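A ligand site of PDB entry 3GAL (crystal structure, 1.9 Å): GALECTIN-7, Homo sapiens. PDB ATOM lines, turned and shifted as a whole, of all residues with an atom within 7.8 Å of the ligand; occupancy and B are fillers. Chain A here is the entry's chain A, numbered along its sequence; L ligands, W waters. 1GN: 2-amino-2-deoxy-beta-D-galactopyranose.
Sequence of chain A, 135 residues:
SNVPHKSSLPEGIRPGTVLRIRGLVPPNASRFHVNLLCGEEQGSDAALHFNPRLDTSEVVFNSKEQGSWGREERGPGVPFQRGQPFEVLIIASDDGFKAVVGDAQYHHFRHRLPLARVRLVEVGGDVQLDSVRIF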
ATOM      1  N   ARG A  31     -29.758 -18.655 -35.643  1.00  0.00           N
ATOM      2  CA  ARG A  31     -29.300 -19.315 -34.396  1.00  0.00           C
ATOM      3  C   ARG A  31     -27.856 -19.020 -34.020  1.00  0.00           C
ATOM      4  O   ARG A  31     -27.037 -18.638 -34.872  1.00  0.00           O
ATOM      5  CB  ARG A  31     -29.481 -20.847 -34.455  1.00  0.00           C
ATOM      6  CG  ARG A  31     -28.984 -21.532 -35.698  1.00  0.00           C
ATOM      7  CD  ARG A  31     -29.195 -23.048 -35.629  1.00  0.00           C
ATOM      8  NE  ARG A  31     -30.578 -23.445 -35.858  1.00  0.00           N
ATOM      9  CZ  ARG A  31     -30.972 -24.708 -36.014  1.00  0.00           C
ATOM     10  NH1 ARG A  31     -30.060 -25.685 -35.953  1.00  0.00           N
ATOM     11  NH2 ARG A  31     -32.243 -25.004 -36.238  1.00  0.00           N
ATOM     12  N   PHE A  32     -27.541 -19.163 -32.729  1.00  0.00           N
ATOM     13  CA  PHE A  32     -26.161 -18.961 -32.250  1.00  0.00           C
ATOM     14  C   PHE A  32     -25.886 -19.971 -31.149  1.00  0.00           C
ATOM     15  O   PHE A  32     -26.798 -20.646 -30.681  1.00  0.00           O
ATOM     16  CB  PHE A  32     -25.910 -17.507 -31.803  1.00  0.00           C
ATOM     17  CG  PHE A  32     -26.650 -17.095 -30.564  1.00  0.00           C
ATOM     18  CD1 PHE A  32     -27.971 -16.644 -30.638  1.00  0.00           C
ATOM     19  CD2 PHE A  32     -26.005 -17.082 -29.326  1.00  0.00           C
ATOM     20  CE1 PHE A  32     -28.632 -16.190 -29.489  1.00  0.00           C
ATOM     21  CE2 PHE A  32     -26.652 -16.617 -28.162  1.00  0.00           C
ATOM     22  CZ  PHE A  32     -27.973 -16.166 -28.250  1.00  0.00           C
ATOM     23  N   HIS A  33     -24.633 -20.120 -30.758  1.00  0.00           N
ATOM     24  CA  HIS A  33     -24.349 -21.098 -29.734  1.00  0.00           C
ATOM     25  C   HIS A  33     -23.164 -20.708 -28.873  1.00  0.00           C
ATOM     26  O   HIS A  33     -22.348 -19.876 -29.262  1.00  0.00           O
ATOM     27  CB  HIS A  33     -24.053 -22.450 -30.373  1.00  0.00           C
ATOM     28  CG  HIS A  33     -22.833 -22.422 -31.238  1.00  0.00           C
ATOM     29  ND1 HIS A  33     -22.892 -22.233 -32.594  1.00  0.00           N
ATOM     30  CD2 HIS A  33     -21.510 -22.448 -30.914  1.00  0.00           C
ATOM     31  CE1 HIS A  33     -21.667 -22.133 -33.075  1.00  0.00           C
ATOM     32  NE2 HIS A  33     -20.809 -22.261 -32.084  1.00  0.00           N
ATOM     33  N   ASN A  35     -20.256 -22.839 -26.716  1.00  0.00           N
ATOM     34  CA  ASN A  35     -19.752 -24.177 -26.473  1.00  0.00           C
ATOM     35  C   ASN A  35     -18.665 -24.102 -25.423  1.00  0.00           C
ATOM     36  O   ASN A  35     -17.887 -23.170 -25.415  1.00  0.00           O
ATOM     37  CB  ASN A  35     -19.129 -24.769 -27.754  1.00  0.00           C
ATOM     38  CG  ASN A  35     -20.141 -25.062 -28.849  1.00  0.00           C
ATOM     39  OD1 ASN A  35     -21.280 -25.426 -28.577  1.00  0.00           O
ATOM     40  ND2 ASN A  35     -19.735 -24.898 -30.097  1.00  0.00           N
ATOM     41  N   HIS A  49     -23.091 -27.533 -25.011  1.00  0.00           N
ATOM     42  CA  HIS A  49     -23.479 -26.842 -26.242  1.00  0.00           C
ATOM     43  C   HIS A  49     -24.820 -26.171 -25.880  1.00  0.00           C
ATOM     44  O   HIS A  49     -25.820 -26.844 -25.590  1.00  0.00           O
ATOM     45  CB  HIS A  49     -23.658 -27.840 -27.392  1.00  0.00           C
ATOM     46  CG  HIS A  49     -24.207 -27.241 -28.664  1.00  0.00           C
ATOM     47  ND1 HIS A  49     -23.489 -26.363 -29.443  1.00  0.00           N
ATOM     48  CD2 HIS A  49     -25.371 -27.456 -29.323  1.00  0.00           C
ATOM     49  CE1 HIS A  49     -24.185 -26.060 -30.519  1.00  0.00           C
ATOM     50  NE2 HIS A  49     -25.329 -26.710 -30.480  1.00  0.00           N
ATOM     51  N   PHE A  50     -24.841 -24.842 -25.837  1.00  0.00           N
ATOM     52  CA  PHE A  50     -26.034 -24.078 -25.505  1.00  0.00           C
ATOM     53  C   PHE A  50     -26.412 -23.435 -26.829  1.00  0.00           C
ATOM     54  O   PHE A  50     -25.693 -22.562 -27.332  1.00  0.00           O
ATOM     55  CB  PHE A  50     -25.670 -23.035 -24.421  1.00  0.00           C
ATOM     56  CG  PHE A  50     -26.724 -21.977 -24.193  1.00  0.00           C
ATOM     57  CD1 PHE A  50     -27.921 -22.290 -23.546  1.00  0.00           C
ATOM     58  CD2 PHE A  50     -26.503 -20.654 -24.577  1.00  0.00           C
ATOM     59  CE1 PHE A  50     -28.861 -21.300 -23.289  1.00  0.00           C
ATOM     60  CE2 PHE A  50     -27.450 -19.655 -24.312  1.00  0.00           C
ATOM     61  CZ  PHE A  50     -28.626 -19.977 -23.672  1.00  0.00           C
ATOM     62  N   ASN A  51     -27.561 -23.841 -27.378  1.00  0.00           N
ATOM     63  CA  ASN A  51     -27.957 -23.388 -28.714  1.00  0.00           C
ATOM     64  C   ASN A  51     -29.328 -22.715 -28.933  1.00  0.00           C
ATOM     65  O   ASN A  51     -30.308 -23.373 -29.300  1.00  0.00           O
ATOM     66  CB  ASN A  51     -27.778 -24.616 -29.628  1.00  0.00           C
ATOM     67  CG  ASN A  51     -27.991 -24.348 -31.098  1.00  0.00           C
ATOM     68  OD1 ASN A  51     -28.415 -25.249 -31.820  1.00  0.00           O
ATOM     69  ND2 ASN A  51     -27.674 -23.142 -31.575  1.00  0.00           N
ATOM     70  N   ARG A  53     -32.183 -21.260 -30.799  1.00  0.00           N
ATOM     71  CA  ARG A  53     -32.569 -21.345 -32.217  1.00  0.00           C
ATOM     72  C   ARG A  53     -33.780 -20.468 -32.478  1.00  0.00           C
ATOM     73  O   ARG A  53     -34.905 -20.853 -32.149  1.00  0.00           O
ATOM     74  CB  ARG A  53     -32.920 -22.782 -32.610  1.00  0.00           C
ATOM     75  CG  ARG A  53     -31.785 -23.759 -32.431  1.00  0.00           C
ATOM     76  CD  ARG A  53     -32.219 -25.183 -32.577  1.00  0.00           C
ATOM     77  NE  ARG A  53     -31.061 -26.066 -32.530  1.00  0.00           N
ATOM     78  CZ  ARG A  53     -31.094 -27.394 -32.645  1.00  0.00           C
ATOM     79  NH1 ARG A  53     -32.241 -28.019 -32.824  1.00  0.00           N
ATOM     80  NH2 ARG A  53     -29.960 -28.098 -32.588  1.00  0.00           N
ATOM     81  N   VAL A  60     -31.699 -25.400 -27.273  1.00  0.00           N
ATOM     82  CA  VAL A  60     -31.230 -26.748 -27.052  1.00  0.00           C
ATOM     83  C   VAL A  60     -29.915 -26.814 -26.276  1.00  0.00           C
ATOM     84  O   VAL A  60     -29.041 -25.966 -26.444  1.00  0.00           O
ATOM     85  CB  VAL A  60     -31.076 -27.486 -28.423  1.00  0.00           C
ATOM     86  CG1 VAL A  60     -30.557 -28.892 -28.224  1.00  0.00           C
ATOM     87  CG2 VAL A  60     -32.405 -27.542 -29.117  1.00  0.00           C
ATOM     88  N   PHE A  61     -29.812 -27.831 -25.426  1.00  0.00           N
ATOM     89  CA  PHE A  61     -28.630 -28.070 -24.593  1.00  0.00           C
ATOM     90  C   PHE A  61     -28.156 -29.486 -24.919  1.00  0.00           C
ATOM     91  O   PHE A  61     -28.961 -30.408 -24.970  1.00  0.00           O
ATOM     92  CB  PHE A  61     -29.002 -28.059 -23.101  1.00  0.00           C
ATOM     93  CG  PHE A  61     -29.324 -26.685 -22.561  1.00  0.00           C
ATOM     94  CD1 PHE A  61     -30.603 -26.163 -22.661  1.00  0.00           C
ATOM     95  CD2 PHE A  61     -28.352 -25.944 -21.895  1.00  0.00           C
ATOM     96  CE1 PHE A  61     -30.910 -24.929 -22.124  1.00  0.00           C
ATOM     97  CE2 PHE A  61     -28.652 -24.700 -21.350  1.00  0.00           C
ATOM     98  CZ  PHE A  61     -29.945 -24.188 -21.465  1.00  0.00           C
ATOM     99  N   ASN A  62     -26.854 -29.681 -25.116  1.00  0.00           N
ATOM    100  CA  ASN A  62     -26.361 -31.018 -25.404  1.00  0.00           C
ATOM    101  C   ASN A  62     -24.872 -31.080 -25.155  1.00  0.00           C
ATOM    102  O   ASN A  62     -24.264 -30.076 -24.872  1.00  0.00           O
ATOM    103  CB  ASN A  62     -26.656 -31.411 -26.869  1.00  0.00           C
ATOM    104  CG  ASN A  62     -26.870 -32.911 -27.033  1.00  0.00           C
ATOM    105  OD1 ASN A  62     -26.494 -33.694 -26.180  1.00  0.00           O
ATOM    106  ND2 ASN A  62     -27.477 -33.307 -28.144  1.00  0.00           N
ATOM    107  N   SER A  63     -24.314 -32.279 -25.254  1.00  0.00           N
ATOM    108  CA  SER A  63     -22.885 -32.500 -25.088  1.00  0.00           C
ATOM    109  C   SER A  63     -22.444 -33.256 -26.348  1.00  0.00           C
ATOM    110  O   SER A  63     -23.269 -33.803 -27.070  1.00  0.00           O
ATOM    111  CB  SER A  63     -22.615 -33.353 -23.856  1.00  0.00           C
ATOM    112  OG  SER A  63     -23.323 -34.572 -23.961  1.00  0.00           O
ATOM    113  N   LYS A  64     -21.151 -33.259 -26.618  1.00  0.00           N
ATOM    114  CA  LYS A  64     -20.627 -33.976 -27.762  1.00  0.00           C
ATOM    115  C   LYS A  64     -19.429 -34.788 -27.309  1.00  0.00           C
ATOM    116  O   LYS A  64     -18.495 -34.276 -26.705  1.00  0.00           O
ATOM    117  CB  LYS A  64     -20.251 -33.006 -28.893  1.00  0.00           C
ATOM    118  CG  LYS A  64     -20.134 -33.695 -30.242  1.00  0.00           C
ATOM    119  CD  LYS A  64     -18.873 -33.319 -30.936  1.00  0.00           C
ATOM    120  CE  LYS A  64     -19.021 -31.977 -31.603  1.00  0.00           C
ATOM    121  NZ  LYS A  64     -17.834 -31.640 -32.420  1.00  0.00           N
ATOM    122  N   TRP A  69     -23.320 -36.343 -30.834  1.00  0.00           N
ATOM    123  CA  TRP A  69     -24.101 -35.525 -29.927  1.00  0.00           C
ATOM    124  C   TRP A  69     -24.870 -36.477 -29.030  1.00  0.00           C
ATOM    125  O   TRP A  69     -25.240 -37.565 -29.444  1.00  0.00           O
ATOM    126  CB  TRP A  69     -25.096 -34.674 -30.700  1.00  0.00           C
ATOM    127  CG  TRP A  69     -24.452 -33.607 -31.462  1.00  0.00           C
ATOM    128  CD1 TRP A  69     -24.233 -33.574 -32.808  1.00  0.00           C
ATOM    129  CD2 TRP A  69     -23.945 -32.379 -30.944  1.00  0.00           C
ATOM    130  NE1 TRP A  69     -23.621 -32.406 -33.166  1.00  0.00           N
ATOM    131  CE2 TRP A  69     -23.423 -31.647 -32.034  1.00  0.00           C
ATOM    132  CE3 TRP A  69     -23.867 -31.816 -29.656  1.00  0.00           C
ATOM    133  CZ2 TRP A  69     -22.838 -30.370 -31.895  1.00  0.00           C
ATOM    134  CZ3 TRP A  69     -23.282 -30.549 -29.517  1.00  0.00           C
ATOM    135  CH2 TRP A  69     -22.781 -29.837 -30.616  1.00  0.00           C
ATOM    136  N   GLY A  70     -25.101 -36.048 -27.794  1.00  0.00           N
ATOM    137  CA  GLY A  70     -25.843 -36.890 -26.881  1.00  0.00           C
ATOM    138  C   GLY A  70     -27.325 -36.592 -26.926  1.00  0.00           C
ATOM    139  O   GLY A  70     -27.848 -36.118 -27.931  1.00  0.00           O
ATOM    140  N   ARG A  71     -28.009 -36.867 -25.815  1.00  0.00           N
ATOM    141  CA  ARG A  71     -29.436 -36.632 -25.705  1.00  0.00           C
ATOM    142  C   ARG A  71     -29.704 -35.130 -25.507  1.00  0.00           C
ATOM    143  O   ARG A  71     -29.139 -34.490 -24.618  1.00  0.00           O
ATOM    144  CB  ARG A  71     -29.985 -37.486 -24.561  1.00  0.00           C
ATOM    145  CG  ARG A  71     -30.998 -36.822 -23.626  1.00  0.00           C
ATOM    146  CD  ARG A  71     -31.908 -37.881 -22.982  1.00  0.00           C
ATOM    147  NE  ARG A  71     -32.979 -38.308 -23.898  1.00  0.00           N
ATOM    148  CZ  ARG A  71     -32.845 -39.215 -24.878  1.00  0.00           C
ATOM    149  NH1 ARG A  71     -31.664 -39.822 -25.086  1.00  0.00           N
ATOM    150  NH2 ARG A  71     -33.878 -39.505 -25.663  1.00  0.00           N
ATOM    151  N   GLU A  72     -30.565 -34.585 -26.355  1.00  0.00           N
ATOM    152  CA  GLU A  72     -30.920 -33.171 -26.310  1.00  0.00           C
ATOM    153  C   GLU A  72     -31.855 -32.841 -25.148  1.00  0.00           C
ATOM    154  O   GLU A  72     -32.735 -33.623 -24.809  1.00  0.00           O
ATOM    155  CB  GLU A  72     -31.599 -32.754 -27.610  1.00  0.00           C
ATOM    156  CG  GLU A  72     -30.669 -32.733 -28.792  1.00  0.00           C
ATOM    157  CD  GLU A  72     -31.316 -32.166 -30.039  1.00  0.00           C
ATOM    158  OE1 GLU A  72     -32.550 -32.253 -30.158  1.00  0.00           O
ATOM    159  OE2 GLU A  72     -30.599 -31.636 -30.903  1.00  0.00           O
ATOM    160  N   GLU A  73     -31.646 -31.681 -24.538  1.00  0.00           N
ATOM    161  CA  GLU A  73     -32.497 -31.188 -23.455  1.00  0.00           C
ATOM    162  C   GLU A  73     -32.924 -29.833 -23.979  1.00  0.00           C
ATOM    163  O   GLU A  73     -32.209 -29.224 -24.771  1.00  0.00           O
ATOM    164  CB  GLU A  73     -31.706 -30.993 -22.175  1.00  0.00           C
ATOM    165  CG  GLU A  73     -31.154 -32.247 -21.604  1.00  0.00           C
ATOM    166  CD  GLU A  73     -30.565 -31.997 -20.242  1.00  0.00           C
ATOM    167  OE1 GLU A  73     -30.770 -30.892 -19.706  1.00  0.00           O
ATOM    168  OE2 GLU A  73     -29.883 -32.888 -19.710  1.00  0.00           O
ATOM    169  N   ARG A  74     -34.093 -29.350 -23.561  1.00  0.00           N
ATOM    170  CA  ARG A  74     -34.570 -28.057 -24.010  1.00  0.00           C
ATOM    171  C   ARG A  74     -35.096 -27.281 -22.822  1.00  0.00           C
ATOM    172  O   ARG A  74     -35.616 -27.860 -21.884  1.00  0.00           O
ATOM    173  CB  ARG A  74     -35.707 -28.214 -25.013  1.00  0.00           C
ATOM    174  CG  ARG A  74     -35.364 -29.032 -26.234  1.00  0.00           C
ATOM    175  CD  ARG A  74     -36.552 -29.130 -27.187  1.00  0.00           C
ATOM    176  NE  ARG A  74     -36.093 -29.053 -28.556  1.00  0.00           N
ATOM    177  CZ  ARG A  74     -35.275 -29.938 -29.124  1.00  0.00           C
ATOM    178  NH1 ARG A  74     -34.842 -30.987 -28.424  1.00  0.00           N
ATOM    179  NH2 ARG A  74     -34.903 -29.795 -30.393  1.00  0.00           N
ATOM    180  N   ARG A 112     -22.065 -34.063 -17.918  1.00  0.00           N
ATOM    181  CA  ARG A 112     -22.009 -35.316 -18.673  1.00  0.00           C
ATOM    182  C   ARG A 112     -20.542 -35.730 -18.807  1.00  0.00           C
ATOM    183  O   ARG A 112     -20.213 -36.916 -18.798  1.00  0.00           O
ATOM    184  CB  ARG A 112     -22.612 -35.116 -20.061  1.00  0.00           C
ATOM    185  CG  ARG A 112     -24.095 -35.290 -20.053  1.00  0.00           C
ATOM    186  CD  ARG A 112     -24.678 -34.731 -21.305  1.00  0.00           C
ATOM    187  NE  ARG A 112     -26.106 -34.476 -21.195  1.00  0.00           N
ATOM    188  CZ  ARG A 112     -26.920 -34.426 -22.243  1.00  0.00           C
ATOM    189  NH1 ARG A 112     -26.424 -34.612 -23.454  1.00  0.00           N
ATOM    190  NH2 ARG A 112     -28.207 -34.170 -22.088  1.00  0.00           N
HETATM  191  C2  1GN L   1     -27.123 -29.533 -34.902  1.00  0.00           C
HETATM  192  C3  1GN L   1     -25.866 -29.212 -34.041  1.00  0.00           C
HETATM  193  C4  1GN L   1     -26.252 -29.120 -32.561  1.00  0.00           C
HETATM  194  O5  1GN L   1     -28.144 -30.621 -33.001  1.00  0.00           O
HETATM  195  C1  1GN L   1     -27.744 -30.815 -34.370  1.00  0.00           C
HETATM  196  O1  1GN L   1     -28.855 -31.136 -35.122  1.00  0.00           O
HETATM  197  N2  1GN L   1     -26.787 -29.687 -36.306  1.00  0.00           N
HETATM  198  O3  1GN L   1     -25.311 -27.974 -34.440  1.00  0.00           O
HETATM  199  O4  1GN L   1     -27.067 -27.977 -32.355  1.00  0.00           O
HETATM  200  C5  1GN L   1     -27.006 -30.391 -32.138  1.00  0.00           C
HETATM  201  C6  1GN L   1     -27.525 -30.341 -30.712  1.00  0.00           C
HETATM  202  O6  1GN L   1     -27.973 -31.617 -30.318  1.00  0.00           O
HETATM  203  O   HOH W   1     -27.386 -25.628 -34.333  1.00  0.00           O
HETATM  204  O   HOH W   2     -22.623 -28.088 -35.024  1.00  0.00           O
HETATM  205  O   HOH W   3     -31.744 -30.854 -33.195  1.00  0.00           O
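OD1 of Asn 62 sits close to O of Arg 71 (3.2 Å). NH1 of Arg 112 sits at hydrogen-bond distance from OD1 of Asn 62 (2.9 Å). The guanidinium group of Arg 53 is in hydrogen-bond range of the side-chain amide oxygen of Asn 51 (2.9 Å). O of Gly 70 sits at hydrogen-bond distance from ND2 of Asn 62. ND2 of Asn 51 lies within hydrogen-bond range of O of Phe 32 (2.8 Å). OE1 of Glu 72 lies within salt-bridge range of NH1 of Arg 74 (3.1 Å). The side-chain amide oxygen of Asn 35 is in hydrogen-bond range of a ring nitrogen (ND1) of His 49. The backbone NH (N) of Asn 51 is in hydrogen-bond range of the backbone carbonyl oxygen (O) of Val 60, at 2.8 Å.
The side-chain carboxylate (OE2) of Glu 72 sits at hydrogen-bond distance from an oxygen (O6) of the ligand, 2.7 Å away. An oxygen (O4) of the ligand lies within hydrogen-bond range of the side-chain amide oxygen (OD1) of Asn 51 (3.1 Å). The side-chain amide nitrogen (ND2) of Asn 62 lies within hydrogen-bond range of an oxygen (O6) of the ligand (2.8 Å). An oxygen (O4) of the ligand lies within hydrogen-bond range of the guanidinium group (NH2) of Arg 53 (2.9 Å). A ring nitrogen (NE2) of His 49 sits at hydrogen-bond distance from an oxygen (O4) of the ligand (2.9 Å).
Residues that only touch the ligand: Trp 69. Hydrophobic or aromatic side chains that line the ligand: His 49 and Trp 69.
Water W1 lies within hydrogen-bond range of OD1 of Asn 51 (2.7 Å), O4 of the ligand (3.1 Å) and NH1 of Arg 31 (3.1 Å). Water W3 lies within hydrogen-bond range of the side-chain carboxylate of Glu 72, the guanidinium group of Arg 53 and an oxygen (O1) of the ligand.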
